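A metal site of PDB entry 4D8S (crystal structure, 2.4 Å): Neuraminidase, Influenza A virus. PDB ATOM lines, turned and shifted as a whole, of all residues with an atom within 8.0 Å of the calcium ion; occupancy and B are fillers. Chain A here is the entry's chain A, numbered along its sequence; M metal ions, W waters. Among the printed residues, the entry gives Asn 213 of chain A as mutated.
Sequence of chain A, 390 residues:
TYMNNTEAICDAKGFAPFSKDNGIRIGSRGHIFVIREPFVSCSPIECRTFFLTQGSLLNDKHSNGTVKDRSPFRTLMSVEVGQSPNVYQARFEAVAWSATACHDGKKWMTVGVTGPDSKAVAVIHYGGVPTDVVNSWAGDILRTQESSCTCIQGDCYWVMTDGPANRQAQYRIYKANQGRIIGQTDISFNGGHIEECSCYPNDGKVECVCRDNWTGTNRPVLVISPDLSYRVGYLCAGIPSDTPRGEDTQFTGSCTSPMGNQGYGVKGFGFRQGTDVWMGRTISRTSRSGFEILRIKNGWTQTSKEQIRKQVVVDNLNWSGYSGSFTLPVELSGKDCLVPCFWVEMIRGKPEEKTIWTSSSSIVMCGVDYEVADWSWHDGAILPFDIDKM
Residues that only touch the calcium ion: Gly 265 (3.7 Å). Five residues have an atom within 4 Å of the calcium ion: Asp 212, Gly 216, Asp 242, Tyr 264 and Gly 265. Along chain A the residues within 4 Å of the calcium ion span positions 212 to 265. The nearest printed residue that does not touch the calcium ion is Asn 213 (4.1 Å).
Water W1 lies within hydrogen-bond range of the backbone carbonyl oxygen of Gly 263 (2.8 Å) and the backbone carbonyl oxygen of Pro 244 (3.0 Å).
O of Tyr 264 sits close to OD1 of Asn 213, at 3.5 Å. The side-chain carboxylate (OD2) of Asp 212 is in hydrogen-bond range of the backbone NH (N) of Trp 214 (3.2 Å). The side-chain carboxylate (OD2) of Asp 212 sits at hydrogen-bond distance from the backbone NH (N) of Thr 215. The side-chain carboxylate (OD2) of Asp 242 is in hydrogen-bond range of the backbone NH (N) of Val 266 (3.2 Å). OD2 of Asp 242 is in salt-bridge range of NH1 of Arg 219. O of Asp 242 is in hydrogen-bond range of NH2 of Arg 245, at 2.9 Å. The backbone NH (N) of Gly 265 sits at hydrogen-bond distance from the side-chain amide oxygen (OD1) of Asn 213, at 3.1 Å. The backbone carbonyl oxygen (O) of Gly 265 sits at hydrogen-bond distance from the guanidinium group (NH1) of Arg 211.
The calcium ion is bound by the backbone carbonyl oxygen (O) of Tyr 264, the backbone carbonyl oxygen (O) of Asp 212, the backbone carbonyl oxygen (O) of Gly 216, water W1 and the side-chain carboxylate (OD1) of Asp 242.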
ATOM      1  N   HIS A 193      10.226 -10.926  21.914  1.00  0.00           N
ATOM      2  CA  HIS A 193      11.012 -10.189  22.894  1.00  0.00           C
ATOM      3  C   HIS A 193      10.172  -9.778  24.095  1.00  0.00           C
ATOM      4  O   HIS A 193       9.267  -8.938  23.984  1.00  0.00           O
ATOM      5  CB  HIS A 193      11.677  -8.959  22.270  1.00  0.00           C
ATOM      6  CG  HIS A 193      12.849  -8.463  23.064  1.00  0.00           C
ATOM      7  ND1 HIS A 193      13.138  -7.126  23.194  1.00  0.00           N
ATOM      8  CD2 HIS A 193      13.796  -9.125  23.762  1.00  0.00           C
ATOM      9  CE1 HIS A 193      14.211  -6.985  23.950  1.00  0.00           C
ATOM     10  NE2 HIS A 193      14.629  -8.187  24.307  1.00  0.00           N
ATOM     11  N   CYS A 210       3.595  -7.992  28.689  1.00  0.00           N
ATOM     12  CA  CYS A 210       4.987  -7.552  28.714  1.00  0.00           C
ATOM     13  C   CYS A 210       5.372  -6.579  27.586  1.00  0.00           C
ATOM     14  O   CYS A 210       4.510  -6.108  26.836  1.00  0.00           O
ATOM     15  CB  CYS A 210       5.923  -8.756  28.704  1.00  0.00           C
ATOM     16  SG  CYS A 210       5.378 -10.144  29.727  1.00  0.00           S
ATOM     17  N   ARG A 211       6.661  -6.293  27.480  1.00  0.00           N
ATOM     18  CA  ARG A 211       7.181  -5.310  26.526  1.00  0.00           C
ATOM     19  C   ARG A 211       8.103  -5.863  25.430  1.00  0.00           C
ATOM     20  O   ARG A 211       9.238  -6.289  25.691  1.00  0.00           O
ATOM     21  CB  ARG A 211       7.937  -4.267  27.342  1.00  0.00           C
ATOM     22  CG  ARG A 211       8.929  -3.436  26.519  1.00  0.00           C
ATOM     23  CD  ARG A 211       9.784  -2.538  27.425  1.00  0.00           C
ATOM     24  NE  ARG A 211      10.518  -1.509  26.682  1.00  0.00           N
ATOM     25  CZ  ARG A 211      11.166  -0.500  27.250  1.00  0.00           C
ATOM     26  NH1 ARG A 211      11.803   0.393  26.501  1.00  0.00           N
ATOM     27  NH2 ARG A 211      11.170  -0.365  28.574  1.00  0.00           N
ATOM     28  N   ASP A 212       7.626  -5.846  24.186  1.00  0.00           N
ATOM     29  CA  ASP A 212       8.453  -6.216  23.061  1.00  0.00           C
ATOM     30  C   ASP A 212       9.291  -4.970  22.747  1.00  0.00           C
ATOM     31  O   ASP A 212       8.750  -3.958  22.315  1.00  0.00           O
ATOM     32  CB  ASP A 212       7.570  -6.617  21.879  1.00  0.00           C
ATOM     33  CG  ASP A 212       8.309  -7.439  20.837  1.00  0.00           C
ATOM     34  OD1 ASP A 212       7.746  -8.478  20.408  1.00  0.00           O
ATOM     35  OD2 ASP A 212       9.419  -7.055  20.422  1.00  0.00           O
ATOM     36  N   ASN A 213      10.591  -5.039  22.991  1.00  0.00           N
ATOM     37  CA  ASN A 213      11.457  -3.879  22.788  1.00  0.00           C
ATOM     38  C   ASN A 213      12.234  -4.016  21.477  1.00  0.00           C
ATOM     39  O   ASN A 213      13.154  -3.249  21.197  1.00  0.00           O
ATOM     40  CB  ASN A 213      12.404  -3.706  23.973  1.00  0.00           C
ATOM     41  CG  ASN A 213      12.937  -2.282  24.093  1.00  0.00           C
ATOM     42  OD1 ASN A 213      12.058  -1.354  24.440  1.00  0.00           O
ATOM     43  ND2 ASN A 213      14.123  -2.034  23.864  1.00  0.00           N
ATOM     44  N   TRP A 214      11.860  -5.037  20.719  1.00  0.00           N
ATOM     45  CA  TRP A 214      12.514  -5.340  19.462  1.00  0.00           C
ATOM     46  C   TRP A 214      11.699  -4.800  18.306  1.00  0.00           C
ATOM     47  O   TRP A 214      12.078  -3.813  17.678  1.00  0.00           O
ATOM     48  CB  TRP A 214      12.719  -6.847  19.314  1.00  0.00           C
ATOM     49  CG  TRP A 214      13.501  -7.236  18.097  1.00  0.00           C
ATOM     50  CD1 TRP A 214      14.056  -6.388  17.182  1.00  0.00           C
ATOM     51  CD2 TRP A 214      13.819  -8.554  17.667  1.00  0.00           C
ATOM     52  NE1 TRP A 214      14.703  -7.108  16.203  1.00  0.00           N
ATOM     53  CE2 TRP A 214      14.574  -8.448  16.486  1.00  0.00           C
ATOM     54  CE3 TRP A 214      13.546  -9.837  18.174  1.00  0.00           C
ATOM     55  CZ2 TRP A 214      15.051  -9.558  15.789  1.00  0.00           C
ATOM     56  CZ3 TRP A 214      14.027 -10.933  17.485  1.00  0.00           C
ATOM     57  CH2 TRP A 214      14.765 -10.793  16.304  1.00  0.00           C
ATOM     58  N   THR A 215      10.583  -5.466  18.003  1.00  0.00           N
ATOM     59  CA  THR A 215       9.790  -5.073  16.844  1.00  0.00           C
ATOM     60  C   THR A 215       8.310  -4.892  17.165  1.00  0.00           C
ATOM     61  O   THR A 215       7.587  -4.281  16.372  1.00  0.00           O
ATOM     62  CB  THR A 215       9.944  -6.100  15.697  1.00  0.00           C
ATOM     63  OG1 THR A 215       9.568  -5.487  14.459  1.00  0.00           O
ATOM     64  CG2 THR A 215       9.074  -7.323  15.946  1.00  0.00           C
ATOM     65  N   GLY A 216       7.862  -5.415  18.295  1.00  0.00           N
ATOM     66  CA  GLY A 216       6.449  -5.361  18.627  1.00  0.00           C
ATOM     67  C   GLY A 216       5.914  -4.052  19.186  1.00  0.00           C
ATOM     68  O   GLY A 216       6.467  -3.490  20.131  1.00  0.00           O
ATOM     69  N   THR A 217       4.837  -3.556  18.589  1.00  0.00           N
ATOM     70  CA  THR A 217       4.096  -2.446  19.194  1.00  0.00           C
ATOM     71  C   THR A 217       2.951  -3.073  19.971  1.00  0.00           C
ATOM     72  O   THR A 217       2.340  -2.420  20.817  1.00  0.00           O
ATOM     73  CB  THR A 217       3.564  -1.452  18.155  1.00  0.00           C
ATOM     74  OG1 THR A 217       3.095  -2.162  17.012  1.00  0.00           O
ATOM     75  CG2 THR A 217       4.666  -0.500  17.718  1.00  0.00           C
ATOM     76  N   ASN A 218       2.660  -4.328  19.671  1.00  0.00           N
ATOM     77  CA  ASN A 218       1.757  -5.132  20.497  1.00  0.00           C
ATOM     78  C   ASN A 218       2.557  -5.862  21.593  1.00  0.00           C
ATOM     79  O   ASN A 218       3.775  -6.036  21.465  1.00  0.00           O
ATOM     80  CB  ASN A 218       0.950  -6.123  19.657  1.00  0.00           C
ATOM     81  CG  ASN A 218       1.824  -7.037  18.805  1.00  0.00           C
ATOM     82  OD1 ASN A 218       2.894  -6.640  18.345  1.00  0.00           O
ATOM     83  ND2 ASN A 218       1.361  -8.270  18.597  1.00  0.00           N
ATOM     84  N   ARG A 219       1.883  -6.289  22.649  1.00  0.00           N
ATOM     85  CA  ARG A 219       2.586  -6.763  23.845  1.00  0.00           C
ATOM     86  C   ARG A 219       2.695  -8.275  23.973  1.00  0.00           C
ATOM     87  O   ARG A 219       1.706  -8.983  23.852  1.00  0.00           O
ATOM     88  CB  ARG A 219       1.939  -6.207  25.102  1.00  0.00           C
ATOM     89  CG  ARG A 219       1.984  -4.697  25.224  1.00  0.00           C
ATOM     90  CD  ARG A 219       1.631  -4.228  26.629  1.00  0.00           C
ATOM     91  NE  ARG A 219       1.857  -2.791  26.744  1.00  0.00           N
ATOM     92  CZ  ARG A 219       3.056  -2.237  26.849  1.00  0.00           C
ATOM     93  NH1 ARG A 219       3.181  -0.914  26.948  1.00  0.00           N
ATOM     94  NH2 ARG A 219       4.135  -3.003  26.839  1.00  0.00           N
ATOM     95  N   PRO A 220       3.910  -8.768  24.234  1.00  0.00           N
ATOM     96  CA  PRO A 220       4.003 -10.182  24.581  1.00  0.00           C
ATOM     97  C   PRO A 220       3.001 -10.517  25.674  1.00  0.00           C
ATOM     98  O   PRO A 220       2.607  -9.638  26.439  1.00  0.00           O
ATOM     99  CB  PRO A 220       5.440 -10.322  25.091  1.00  0.00           C
ATOM    100  CG  PRO A 220       6.187  -9.263  24.350  1.00  0.00           C
ATOM    101  CD  PRO A 220       5.223  -8.111  24.190  1.00  0.00           C
ATOM    102  N   ASP A 242       1.618  -0.292  22.986  1.00  0.00           N
ATOM    103  CA  ASP A 242       3.013   0.077  23.284  1.00  0.00           C
ATOM    104  C   ASP A 242       3.338   1.517  22.860  1.00  0.00           C
ATOM    105  O   ASP A 242       2.490   2.216  22.300  1.00  0.00           O
ATOM    106  CB  ASP A 242       3.981  -0.929  22.630  1.00  0.00           C
ATOM    107  CG  ASP A 242       5.275  -1.105  23.429  1.00  0.00           C
ATOM    108  OD1 ASP A 242       6.181  -1.844  22.964  1.00  0.00           O
ATOM    109  OD2 ASP A 242       5.373  -0.510  24.533  1.00  0.00           O
ATOM    110  N   THR A 243       4.556   1.957  23.135  1.00  0.00           N
ATOM    111  CA  THR A 243       5.017   3.298  22.756  1.00  0.00           C
ATOM    112  C   THR A 243       6.522   3.287  22.490  1.00  0.00           C
ATOM    113  O   THR A 243       7.280   2.867  23.365  1.00  0.00           O
ATOM    114  CB  THR A 243       4.750   4.325  23.880  1.00  0.00           C
ATOM    115  OG1 THR A 243       3.388   4.217  24.317  1.00  0.00           O
ATOM    116  CG2 THR A 243       5.034   5.736  23.400  1.00  0.00           C
ATOM    117  N   PRO A 244       6.953   3.742  21.297  1.00  0.00           N
ATOM    118  CA  PRO A 244       6.126   4.225  20.191  1.00  0.00           C
ATOM    119  C   PRO A 244       5.313   3.125  19.502  1.00  0.00           C
ATOM    120  O   PRO A 244       5.628   1.933  19.606  1.00  0.00           O
ATOM    121  CB  PRO A 244       7.153   4.790  19.201  1.00  0.00           C
ATOM    122  CG  PRO A 244       8.381   4.031  19.483  1.00  0.00           C
ATOM    123  CD  PRO A 244       8.388   3.849  20.969  1.00  0.00           C
ATOM    124  N   ARG A 245       4.267   3.557  18.802  1.00  0.00           N
ATOM    125  CA  ARG A 245       3.365   2.652  18.117  1.00  0.00           C
ATOM    126  C   ARG A 245       2.793   3.369  16.910  1.00  0.00           C
ATOM    127  O   ARG A 245       2.987   4.564  16.732  1.00  0.00           O
ATOM    128  CB  ARG A 245       2.215   2.246  19.049  1.00  0.00           C
ATOM    129  CG  ARG A 245       1.357   3.432  19.503  1.00  0.00           C
ATOM    130  CD  ARG A 245       0.201   2.967  20.376  1.00  0.00           C
ATOM    131  NE  ARG A 245      -0.604   4.087  20.853  1.00  0.00           N
ATOM    132  CZ  ARG A 245      -0.347   4.783  21.963  1.00  0.00           C
ATOM    133  NH1 ARG A 245      -1.142   5.780  22.317  1.00  0.00           N
ATOM    134  NH2 ARG A 245       0.704   4.491  22.708  1.00  0.00           N
ATOM    135  N   MET A 259       3.751  -7.289  15.806  1.00  0.00           N
ATOM    136  CA  MET A 259       3.261  -6.483  14.697  1.00  0.00           C
ATOM    137  C   MET A 259       3.765  -5.046  14.788  1.00  0.00           C
ATOM    138  O   MET A 259       4.131  -4.574  15.853  1.00  0.00           O
ATOM    139  CB  MET A 259       1.727  -6.518  14.650  1.00  0.00           C
ATOM    140  CG  MET A 259       1.163  -7.869  14.255  1.00  0.00           C
ATOM    141  SD  MET A 259       1.485  -8.268  12.522  1.00  0.00           S
ATOM    142  CE  MET A 259       0.675  -6.865  11.732  1.00  0.00           C
ATOM    143  N   GLN A 262       8.224  -1.023  14.588  1.00  0.00           N
ATOM    144  CA  GLN A 262       8.767  -0.083  15.546  1.00  0.00           C
ATOM    145  C   GLN A 262       9.669  -0.755  16.568  1.00  0.00           C
ATOM    146  O   GLN A 262       9.308  -1.759  17.180  1.00  0.00           O
ATOM    147  CB  GLN A 262       7.636   0.679  16.251  1.00  0.00           C
ATOM    148  CG  GLN A 262       7.076   1.867  15.465  1.00  0.00           C
ATOM    149  CD  GLN A 262       8.107   2.985  15.280  1.00  0.00           C
ATOM    150  OE1 GLN A 262       9.322   2.759  15.378  1.00  0.00           O
ATOM    151  NE2 GLN A 262       7.619   4.201  15.033  1.00  0.00           N
ATOM    152  N   GLY A 263      10.860  -0.193  16.732  1.00  0.00           N
ATOM    153  CA  GLY A 263      11.734  -0.575  17.822  1.00  0.00           C
ATOM    154  C   GLY A 263      11.346   0.199  19.079  1.00  0.00           C
ATOM    155  O   GLY A 263      10.432   1.016  19.042  1.00  0.00           O
ATOM    156  N   TYR A 264      12.055  -0.057  20.175  1.00  0.00           N
ATOM    157  CA  TYR A 264      11.784   0.611  21.441  1.00  0.00           C
ATOM    158  C   TYR A 264      10.543   0.060  22.113  1.00  0.00           C
ATOM    159  O   TYR A 264       9.985  -0.964  21.692  1.00  0.00           O
ATOM    160  CB  TYR A 264      11.670   2.121  21.252  1.00  0.00           C
ATOM    161  CG  TYR A 264      12.894   2.729  20.631  1.00  0.00           C
ATOM    162  CD1 TYR A 264      13.888   3.285  21.429  1.00  0.00           C
ATOM    163  CD2 TYR A 264      13.075   2.742  19.254  1.00  0.00           C
ATOM    164  CE1 TYR A 264      15.020   3.837  20.874  1.00  0.00           C
ATOM    165  CE2 TYR A 264      14.201   3.293  18.691  1.00  0.00           C
ATOM    166  CZ  TYR A 264      15.180   3.839  19.502  1.00  0.00           C
ATOM    167  OH  TYR A 264      16.305   4.396  18.952  1.00  0.00           O
ATOM    168  N   GLY A 265      10.099   0.753  23.158  1.00  0.00           N
ATOM    169  CA  GLY A 265       8.913   0.382  23.911  1.00  0.00           C
ATOM    170  C   GLY A 265       8.877   1.024  25.281  1.00  0.00           C
ATOM    171  O   GLY A 265       9.629   1.952  25.582  1.00  0.00           O
ATOM    172  N   VAL A 266       7.976   0.520  26.125  1.00  0.00           N
ATOM    173  CA  VAL A 266       7.826   0.988  27.491  1.00  0.00           C
ATOM    174  C   VAL A 266       6.952   0.007  28.258  1.00  0.00           C
ATOM    175  O   VAL A 266       6.069  -0.626  27.682  1.00  0.00           O
ATOM    176  CB  VAL A 266       7.179   2.388  27.541  1.00  0.00           C
ATOM    177  CG1 VAL A 266       5.785   2.345  26.921  1.00  0.00           C
ATOM    178  CG2 VAL A 266       7.131   2.901  28.963  1.00  0.00           C
HETATM  179 CA    CA M   1       8.097  -2.064  21.289  1.00  0.00          CA
HETATM  180  O   HOH W   1       8.020   0.119  20.089  1.00  0.00           O
